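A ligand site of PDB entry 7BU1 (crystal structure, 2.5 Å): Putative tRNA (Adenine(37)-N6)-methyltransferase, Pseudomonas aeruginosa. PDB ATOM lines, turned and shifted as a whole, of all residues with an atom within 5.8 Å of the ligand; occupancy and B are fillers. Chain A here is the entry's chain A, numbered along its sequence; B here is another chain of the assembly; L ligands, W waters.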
ATOM      1  N   LYS A  24      10.007 -19.771 -16.837  1.00  0.00           N
ATOM      2  CA  LYS A  24      10.706 -18.724 -16.094  1.00  0.00           C
ATOM      3  C   LYS A  24       9.740 -17.695 -15.499  1.00  0.00           C
ATOM      4  O   LYS A  24       9.990 -17.165 -14.414  1.00  0.00           O
ATOM      5  CB  LYS A  24      11.733 -18.032 -16.992  1.00  0.00           C
ATOM      6  CG  LYS A  24      12.827 -18.955 -17.534  1.00  0.00           C
ATOM      7  CD  LYS A  24      13.913 -18.221 -18.322  1.00  0.00           C
ATOM      8  CE  LYS A  24      14.941 -17.563 -17.392  1.00  0.00           C
ATOM      9  NZ  LYS A  24      16.181 -17.059 -18.068  1.00  0.00           N
ATOM     10  N   ILE A  27       8.354 -16.816 -11.537  1.00  0.00           N
ATOM     11  CA  ILE A  27       9.182 -17.379 -10.472  1.00  0.00           C
ATOM     12  C   ILE A  27       9.518 -16.258  -9.499  1.00  0.00           C
ATOM     13  O   ILE A  27      10.038 -15.209  -9.928  1.00  0.00           O
ATOM     14  CB  ILE A  27      10.449 -18.020 -11.051  1.00  0.00           C
ATOM     15  CG1 ILE A  27      10.100 -19.335 -11.747  1.00  0.00           C
ATOM     16  CG2 ILE A  27      11.468 -18.268  -9.951  1.00  0.00           C
ATOM     17  CD1 ILE A  27      11.305 -20.062 -12.311  1.00  0.00           C
ATOM     18  N   PRO A  28       9.243 -16.399  -8.203  1.00  0.00           N
ATOM     19  CA  PRO A  28       9.353 -15.241  -7.309  1.00  0.00           C
ATOM     20  C   PRO A  28      10.764 -14.655  -7.294  1.00  0.00           C
ATOM     21  O   PRO A  28      11.764 -15.377  -7.321  1.00  0.00           O
ATOM     22  CB  PRO A  28       8.975 -15.805  -5.934  1.00  0.00           C
ATOM     23  CG  PRO A  28       8.969 -17.292  -6.089  1.00  0.00           C
ATOM     24  CD  PRO A  28       8.667 -17.574  -7.525  1.00  0.00           C
ATOM     25  N   PHE A  66      24.346 -25.246  -9.750  1.00  0.00           N
ATOM     26  CA  PHE A  66      23.594 -25.886 -10.808  1.00  0.00           C
ATOM     27  C   PHE A  66      23.952 -25.251 -12.143  1.00  0.00           C
ATOM     28  O   PHE A  66      24.592 -24.204 -12.214  1.00  0.00           O
ATOM     29  CB  PHE A  66      22.082 -25.778 -10.539  1.00  0.00           C
ATOM     30  CG  PHE A  66      21.571 -24.365 -10.518  1.00  0.00           C
ATOM     31  CD1 PHE A  66      21.630 -23.613  -9.354  1.00  0.00           C
ATOM     32  CD2 PHE A  66      21.050 -23.799 -11.660  1.00  0.00           C
ATOM     33  CE1 PHE A  66      21.162 -22.317  -9.332  1.00  0.00           C
ATOM     34  CE2 PHE A  66      20.581 -22.499 -11.660  1.00  0.00           C
ATOM     35  CZ  PHE A  66      20.645 -21.748 -10.488  1.00  0.00           C
ATOM     36  N   LEU A  67      23.501 -25.901 -13.208  1.00  0.00           N
ATOM     37  CA  LEU A  67      23.712 -25.420 -14.567  1.00  0.00           C
ATOM     38  C   LEU A  67      22.425 -24.794 -15.087  1.00  0.00           C
ATOM     39  O   LEU A  67      21.338 -25.373 -14.949  1.00  0.00           O
ATOM     40  CB  LEU A  67      24.160 -26.554 -15.468  1.00  0.00           C
ATOM     41  CG  LEU A  67      25.535 -27.129 -15.152  1.00  0.00           C
ATOM     42  CD1 LEU A  67      25.807 -28.300 -16.075  1.00  0.00           C
ATOM     43  CD2 LEU A  67      26.610 -26.052 -15.265  1.00  0.00           C
ATOM     44  N   PHE A  68      22.553 -23.623 -15.713  1.00  0.00           N
ATOM     45  CA  PHE A  68      21.418 -22.949 -16.360  1.00  0.00           C
ATOM     46  C   PHE A  68      21.113 -23.653 -17.681  1.00  0.00           C
ATOM     47  O   PHE A  68      21.375 -23.147 -18.779  1.00  0.00           O
ATOM     48  CB  PHE A  68      21.728 -21.475 -16.602  1.00  0.00           C
ATOM     49  CG  PHE A  68      21.806 -20.644 -15.340  1.00  0.00           C
ATOM     50  CD1 PHE A  68      20.664 -20.371 -14.597  1.00  0.00           C
ATOM     51  CD2 PHE A  68      23.017 -20.099 -14.932  1.00  0.00           C
ATOM     52  CE1 PHE A  68      20.736 -19.592 -13.461  1.00  0.00           C
ATOM     53  CE2 PHE A  68      23.080 -19.300 -13.801  1.00  0.00           C
ATOM     54  CZ  PHE A  68      21.952 -19.054 -13.068  1.00  0.00           C
ATOM     55  N   HIS A  69      20.516 -24.843 -17.577  1.00  0.00           N
ATOM     56  CA  HIS A  69      20.372 -25.676 -18.769  1.00  0.00           C
ATOM     57  C   HIS A  69      19.375 -25.101 -19.774  1.00  0.00           C
ATOM     58  O   HIS A  69      19.414 -25.495 -20.950  1.00  0.00           O
ATOM     59  CB  HIS A  69      19.995 -27.114 -18.394  1.00  0.00           C
ATOM     60  CG  HIS A  69      18.583 -27.278 -17.939  1.00  0.00           C
ATOM     61  ND1 HIS A  69      18.048 -26.544 -16.896  1.00  0.00           N
ATOM     62  CD2 HIS A  69      17.599 -28.114 -18.348  1.00  0.00           C
ATOM     63  CE1 HIS A  69      16.795 -26.923 -16.707  1.00  0.00           C
ATOM     64  NE2 HIS A  69      16.503 -27.869 -17.575  1.00  0.00           N
ATOM     65  N   GLN A  70      18.492 -24.177 -19.383  1.00  0.00           N
ATOM     66  CA  GLN A  70      17.577 -23.574 -20.351  1.00  0.00           C
ATOM     67  C   GLN A  70      17.985 -22.154 -20.721  1.00  0.00           C
ATOM     68  O   GLN A  70      17.144 -21.377 -21.201  1.00  0.00           O
ATOM     69  CB  GLN A  70      16.140 -23.581 -19.823  1.00  0.00           C
ATOM     70  CG  GLN A  70      15.704 -24.889 -19.188  1.00  0.00           C
ATOM     71  CD  GLN A  70      14.802 -25.696 -20.086  1.00  0.00           C
ATOM     72  OE1 GLN A  70      14.976 -25.720 -21.306  1.00  0.00           O
ATOM     73  NE2 GLN A  70      13.829 -26.367 -19.492  1.00  0.00           N
ATOM     74  N   ALA A  71      19.251 -21.796 -20.542  1.00  0.00           N
ATOM     75  CA  ALA A  71      19.736 -20.489 -20.952  1.00  0.00           C
ATOM     76  C   ALA A  71      20.724 -20.643 -22.104  1.00  0.00           C
ATOM     77  O   ALA A  71      21.863 -21.045 -21.884  1.00  0.00           O
ATOM     78  CB  ALA A  71      20.393 -19.759 -19.788  1.00  0.00           C
ATOM     79  N   ARG A  97      23.307 -11.408 -11.347  1.00  0.00           N
ATOM     80  CA  ARG A  97      23.061 -12.837 -11.181  1.00  0.00           C
ATOM     81  C   ARG A  97      22.338 -13.424 -12.400  1.00  0.00           C
ATOM     82  O   ARG A  97      21.539 -14.359 -12.244  1.00  0.00           O
ATOM     83  CB  ARG A  97      22.275 -13.103  -9.901  1.00  0.00           C
ATOM     84  CG  ARG A  97      22.898 -12.534  -8.617  1.00  0.00           C
ATOM     85  CD  ARG A  97      24.130 -13.315  -8.147  1.00  0.00           C
ATOM     86  NE  ARG A  97      23.749 -14.504  -7.372  1.00  0.00           N
ATOM     87  CZ  ARG A  97      23.740 -14.585  -6.046  1.00  0.00           C
ATOM     88  NH1 ARG A  97      24.093 -13.554  -5.307  1.00  0.00           N
ATOM     89  NH2 ARG A  97      23.358 -15.710  -5.460  1.00  0.00           N
ATOM     90  N   ALA A  98      22.603 -12.892 -13.589  1.00  0.00           N
ATOM     91  CA  ALA A  98      21.886 -13.304 -14.797  1.00  0.00           C
ATOM     92  C   ALA A  98      22.130 -14.776 -15.088  1.00  0.00           C
ATOM     93  O   ALA A  98      23.119 -15.365 -14.652  1.00  0.00           O
ATOM     94  CB  ALA A  98      22.323 -12.483 -16.000  1.00  0.00           C
ATOM     95  N   THR A  99      21.186 -15.375 -15.808  1.00  0.00           N
ATOM     96  CA  THR A  99      21.307 -16.795 -16.108  1.00  0.00           C
ATOM     97  C   THR A  99      22.124 -17.074 -17.359  1.00  0.00           C
ATOM     98  O   THR A  99      22.509 -18.227 -17.576  1.00  0.00           O
ATOM     99  CB  THR A  99      19.918 -17.410 -16.229  1.00  0.00           C
ATOM    100  OG1 THR A  99      19.244 -16.880 -17.371  1.00  0.00           O
ATOM    101  CG2 THR A  99      19.109 -17.073 -15.000  1.00  0.00           C
ATOM    102  N   ILE A 105      26.858 -21.356 -14.749  1.00  0.00           N
ATOM    103  CA  ILE A 105      26.645 -21.963 -13.434  1.00  0.00           C
ATOM    104  C   ILE A 105      25.819 -21.032 -12.558  1.00  0.00           C
ATOM    105  O   ILE A 105      26.124 -19.838 -12.443  1.00  0.00           O
ATOM    106  CB  ILE A 105      27.976 -22.301 -12.753  1.00  0.00           C
ATOM    107  CG1 ILE A 105      28.734 -23.355 -13.578  1.00  0.00           C
ATOM    108  CG2 ILE A 105      27.725 -22.835 -11.365  1.00  0.00           C
ATOM    109  CD1 ILE A 105      30.178 -23.457 -13.249  1.00  0.00           C
ATOM    110  N   GLY A 106      24.786 -21.585 -11.931  1.00  0.00           N
ATOM    111  CA  GLY A 106      23.969 -20.861 -10.986  1.00  0.00           C
ATOM    112  C   GLY A 106      24.296 -21.244  -9.550  1.00  0.00           C
ATOM    113  O   GLY A 106      24.983 -22.234  -9.290  1.00  0.00           O
ATOM    114  N   GLN A 107      23.773 -20.436  -8.622  1.00  0.00           N
ATOM    115  CA  GLN A 107      24.026 -20.603  -7.196  1.00  0.00           C
ATOM    116  C   GLN A 107      22.789 -20.144  -6.430  1.00  0.00           C
ATOM    117  O   GLN A 107      22.476 -18.955  -6.411  1.00  0.00           O
ATOM    118  CB  GLN A 107      25.256 -19.800  -6.776  1.00  0.00           C
ATOM    119  CG  GLN A 107      25.479 -19.679  -5.264  1.00  0.00           C
ATOM    120  CD  GLN A 107      26.688 -18.808  -4.896  1.00  0.00           C
ATOM    121  OE1 GLN A 107      27.578 -18.576  -5.710  1.00  0.00           O
ATOM    122  NE2 GLN A 107      26.716 -18.344  -3.648  1.00  0.00           N
ATOM    123  N   SER A 108      22.125 -21.070  -5.729  1.00  0.00           N
ATOM    124  CA  SER A 108      20.921 -20.726  -4.980  1.00  0.00           C
ATOM    125  C   SER A 108      20.958 -21.355  -3.599  1.00  0.00           C
ATOM    126  O   SER A 108      21.368 -22.507  -3.440  1.00  0.00           O
ATOM    127  CB  SER A 108      19.640 -21.187  -5.698  1.00  0.00           C
ATOM    128  OG  SER A 108      19.623 -20.797  -7.053  1.00  0.00           O
ATOM    129  N   VAL A 109      20.457 -20.613  -2.620  1.00  0.00           N
ATOM    130  CA  VAL A 109      20.258 -21.122  -1.271  1.00  0.00           C
ATOM    131  C   VAL A 109      18.775 -21.450  -1.122  1.00  0.00           C
ATOM    132  O   VAL A 109      17.916 -20.597  -1.356  1.00  0.00           O
ATOM    133  CB  VAL A 109      20.736 -20.127  -0.204  1.00  0.00           C
ATOM    134  CG1 VAL A 109      20.143 -18.729  -0.413  1.00  0.00           C
ATOM    135  CG2 VAL A 109      20.385 -20.637   1.184  1.00  0.00           C
ATOM    136  N   ASP A 126      14.044 -21.480  -6.543  1.00  0.00           N
ATOM    137  CA  ASP A 126      13.904 -20.655  -7.737  1.00  0.00           C
ATOM    138  C   ASP A 126      14.363 -21.386  -8.989  1.00  0.00           C
ATOM    139  O   ASP A 126      14.684 -20.743  -9.994  1.00  0.00           O
ATOM    140  CB  ASP A 126      14.675 -19.341  -7.560  1.00  0.00           C
ATOM    141  CG  ASP A 126      16.178 -19.562  -7.376  1.00  0.00           C
ATOM    142  OD1 ASP A 126      16.625 -20.728  -7.284  1.00  0.00           O
ATOM    143  OD2 ASP A 126      16.907 -18.544  -7.315  1.00  0.00           O
ATOM    144  N   LEU A 127      14.359 -22.708  -8.971  1.00  0.00           N
ATOM    145  CA  LEU A 127      14.994 -23.495 -10.027  1.00  0.00           C
ATOM    146  C   LEU A 127      13.968 -24.134 -10.945  1.00  0.00           C
ATOM    147  O   LEU A 127      12.956 -24.674 -10.490  1.00  0.00           O
ATOM    148  CB  LEU A 127      15.891 -24.582  -9.421  1.00  0.00           C
ATOM    149  CG  LEU A 127      16.880 -24.007  -8.407  1.00  0.00           C
ATOM    150  CD1 LEU A 127      17.566 -25.121  -7.618  1.00  0.00           C
ATOM    151  CD2 LEU A 127      17.880 -23.137  -9.114  1.00  0.00           C
ATOM    152  N   LEU A 128      14.258 -24.103 -12.247  1.00  0.00           N
ATOM    153  CA  LEU A 128      13.389 -24.715 -13.228  1.00  0.00           C
ATOM    154  C   LEU A 128      13.358 -26.234 -13.051  1.00  0.00           C
ATOM    155  O   LEU A 128      14.298 -26.844 -12.543  1.00  0.00           O
ATOM    156  CB  LEU A 128      13.849 -24.367 -14.643  1.00  0.00           C
ATOM    157  CG  LEU A 128      13.413 -22.989 -15.112  1.00  0.00           C
ATOM    158  CD1 LEU A 128      13.860 -22.722 -16.550  1.00  0.00           C
ATOM    159  CD2 LEU A 128      11.909 -22.857 -14.971  1.00  0.00           C
ATOM    160  N   THR A 131      16.563 -29.146 -13.662  1.00  0.00           N
ATOM    161  CA  THR A 131      17.855 -28.474 -13.608  1.00  0.00           C
ATOM    162  C   THR A 131      18.929 -29.415 -13.076  1.00  0.00           C
ATOM    163  O   THR A 131      18.737 -30.042 -12.038  1.00  0.00           O
ATOM    164  CB  THR A 131      17.814 -27.201 -12.747  1.00  0.00           C
ATOM    165  OG1 THR A 131      16.600 -26.472 -12.968  1.00  0.00           O
ATOM    166  CG2 THR A 131      18.999 -26.315 -13.075  1.00  0.00           C
ATOM    167  N   PRO A 132      20.073 -29.533 -13.762  1.00  0.00           N
ATOM    168  CA  PRO A 132      21.159 -30.386 -13.252  1.00  0.00           C
ATOM    169  C   PRO A 132      21.914 -29.706 -12.123  1.00  0.00           C
ATOM    170  O   PRO A 132      22.334 -28.543 -12.246  1.00  0.00           O
ATOM    171  CB  PRO A 132      22.058 -30.593 -14.486  1.00  0.00           C
ATOM    172  CG  PRO A 132      21.297 -30.001 -15.654  1.00  0.00           C
ATOM    173  CD  PRO A 132      20.389 -28.969 -15.080  1.00  0.00           C
ATOM    174  N   LYS B 137      30.000 -13.462  -8.978  1.00  0.00           N
ATOM    175  CA  LYS B 137      28.603 -13.125  -8.730  1.00  0.00           C
ATOM    176  C   LYS B 137      28.549 -12.046  -7.660  1.00  0.00           C
ATOM    177  O   LYS B 137      29.211 -12.172  -6.604  1.00  0.00           O
ATOM    178  CB  LYS B 137      27.775 -14.332  -8.282  1.00  0.00           C
ATOM    179  CG  LYS B 137      27.497 -15.385  -9.350  1.00  0.00           C
ATOM    180  CD  LYS B 137      27.149 -16.722  -8.697  1.00  0.00           C
ATOM    181  CE  LYS B 137      26.542 -17.722  -9.682  1.00  0.00           C
ATOM    182  NZ  LYS B 137      27.047 -17.526 -11.066  1.00  0.00           N
HETATM  183  N1  LIG L   1      19.940 -17.791  -7.332  1.00  0.00           N
HETATM  184  C1  LIG L   1      20.560 -18.116  -8.628  1.00  0.00           C
HETATM  185  C2  LIG L   1      21.867 -17.323  -8.836  1.00  0.00           C
HETATM  186  O1  LIG L   1      22.705 -17.837  -9.615  1.00  0.00           O
HETATM  187  O2  LIG L   1      21.999 -16.209  -8.255  1.00  0.00           O
HETATM  188  C3  LIG L   1      19.602 -17.836  -9.794  1.00  0.00           C
HETATM  189  C4  LIG L   1      19.492 -16.322 -10.020  1.00  0.00           C
HETATM  190  S1  LIG L   1      18.369 -15.977 -11.422  1.00  0.00           S
HETATM  191  C5  LIG L   1      18.257 -14.214 -11.660  1.00  0.00           C
HETATM  192  C6  LIG L   1      16.711 -16.671 -11.058  1.00  0.00           C
HETATM  193  C7  LIG L   1      16.087 -17.131 -12.378  1.00  0.00           C
HETATM  194  O3  LIG L   1      16.852 -18.204 -12.912  1.00  0.00           O
HETATM  195  C8  LIG L   1      14.785 -17.851 -12.167  1.00  0.00           C
HETATM  196  O4  LIG L   1      13.762 -16.933 -11.756  1.00  0.00           O
HETATM  197  C9  LIG L   1      14.561 -18.299 -13.580  1.00  0.00           C
HETATM  198  O5  LIG L   1      14.297 -17.136 -14.357  1.00  0.00           O
HETATM  199  C10 LIG L   1      15.980 -18.771 -13.921  1.00  0.00           C
HETATM  200  N2  LIG L   1      16.232 -20.223 -13.791  1.00  0.00           N
HETATM  201  C11 LIG L   1      15.965 -21.108 -12.825  1.00  0.00           C
HETATM  202  N3  LIG L   1      16.415 -22.287 -13.239  1.00  0.00           N
HETATM  203  C12 LIG L   1      16.979 -22.123 -14.441  1.00  0.00           C
HETATM  204  C13 LIG L   1      17.575 -22.977 -15.275  1.00  0.00           C
HETATM  205  N4  LIG L   1      17.654 -24.239 -14.874  1.00  0.00           N
HETATM  206  N5  LIG L   1      18.068 -22.583 -16.452  1.00  0.00           N
HETATM  207  C14 LIG L   1      17.960 -21.258 -16.833  1.00  0.00           C
HETATM  208  N6  LIG L   1      17.316 -20.380 -15.947  1.00  0.00           N
HETATM  209  C15 LIG L   1      16.858 -20.848 -14.783  1.00  0.00           C
HETATM  210  O   HOH W   1      19.431 -15.116  -6.177  1.00  0.00           O
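Lys 24 touches the ligand. Ile 27 touches the ligand. Leu 67 touches the ligand (O to N4, 3.9 Å). Phe 68 touches the ligand. Ala 71 touches the ligand. Thr 99 touches the ligand (CG2 to O3, 3.3 Å). CA of Gly 106 touches O1 of the ligand, at 3.6 Å. Leu 127 touches the ligand (CA to N3, 3.7 Å). Lys 137 of chain B touches the ligand. Within 4 Å of the ligand: Lys 24, Ile 27, Leu 67, Phe 68, His 69, Gln 70, Ala 71, Arg 97, Thr 99, Gly 106, Gln 107, Ser 108, Asp 126, Leu 127, Leu 128, Thr 131 and Lys 137 of chain B. The nearest printed residue that does not touch the ligand is Phe 66 (4.1 Å).
An oxygen (O1) of the ligand sits at hydrogen-bond distance from the backbone NH (N) of Gln 107 (3.0 Å). A nitrogen (N4) of the ligand lies close to the side-chain hydroxyl (OG1) of Thr 131. A nitrogen (N1) of the ligand is in hydrogen-bond range of the side-chain hydroxyl (OG) of Ser 108. O of Gln 107 is in hydrogen-bond range of N1 of the ligand (2.9 Å). N of Leu 128 lies within hydrogen-bond range of N3 of the ligand (3.0 Å). A ring nitrogen (ND1) of His 69 is in hydrogen-bond range of a nitrogen (N4) of the ligand, at 3.1 Å. The backbone NH (N) of Gln 70 is in hydrogen-bond range of a nitrogen (N5) of the ligand, 3.4 Å away. NE of Arg 97 lies within salt-bridge range of O2 of the ligand. The side-chain carboxylate (OD2) of Asp 126 is in salt-bridge range of a nitrogen (N1) of the ligand (3.1 Å).
NZ of Lys 137 of chain B sits at hydrogen-bond distance from O of Ile 105 (2.8 Å). The side-chain hydroxyl (OG) of Ser 108 is in hydrogen-bond range of the side-chain carboxylate (OD1) of Asp 126. NZ of Lys 24 sits at hydrogen-bond distance from OG1 of Thr 99. N of Leu 128 sits close to OG1 of Thr 131, 3.4 Å away. The backbone carbonyl oxygen (O) of Gln 107 sits at hydrogen-bond distance from the guanidinium group (NH2) of Arg 97 (3.5 Å). The backbone carbonyl oxygen (O) of Pro 132 lies within hydrogen-bond range of the backbone NH (N) of Leu 67 (3.0 Å). The backbone NH (N) of Gly 106 lies within hydrogen-bond range of the backbone carbonyl oxygen (O) of Phe 66, at 2.6 Å.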
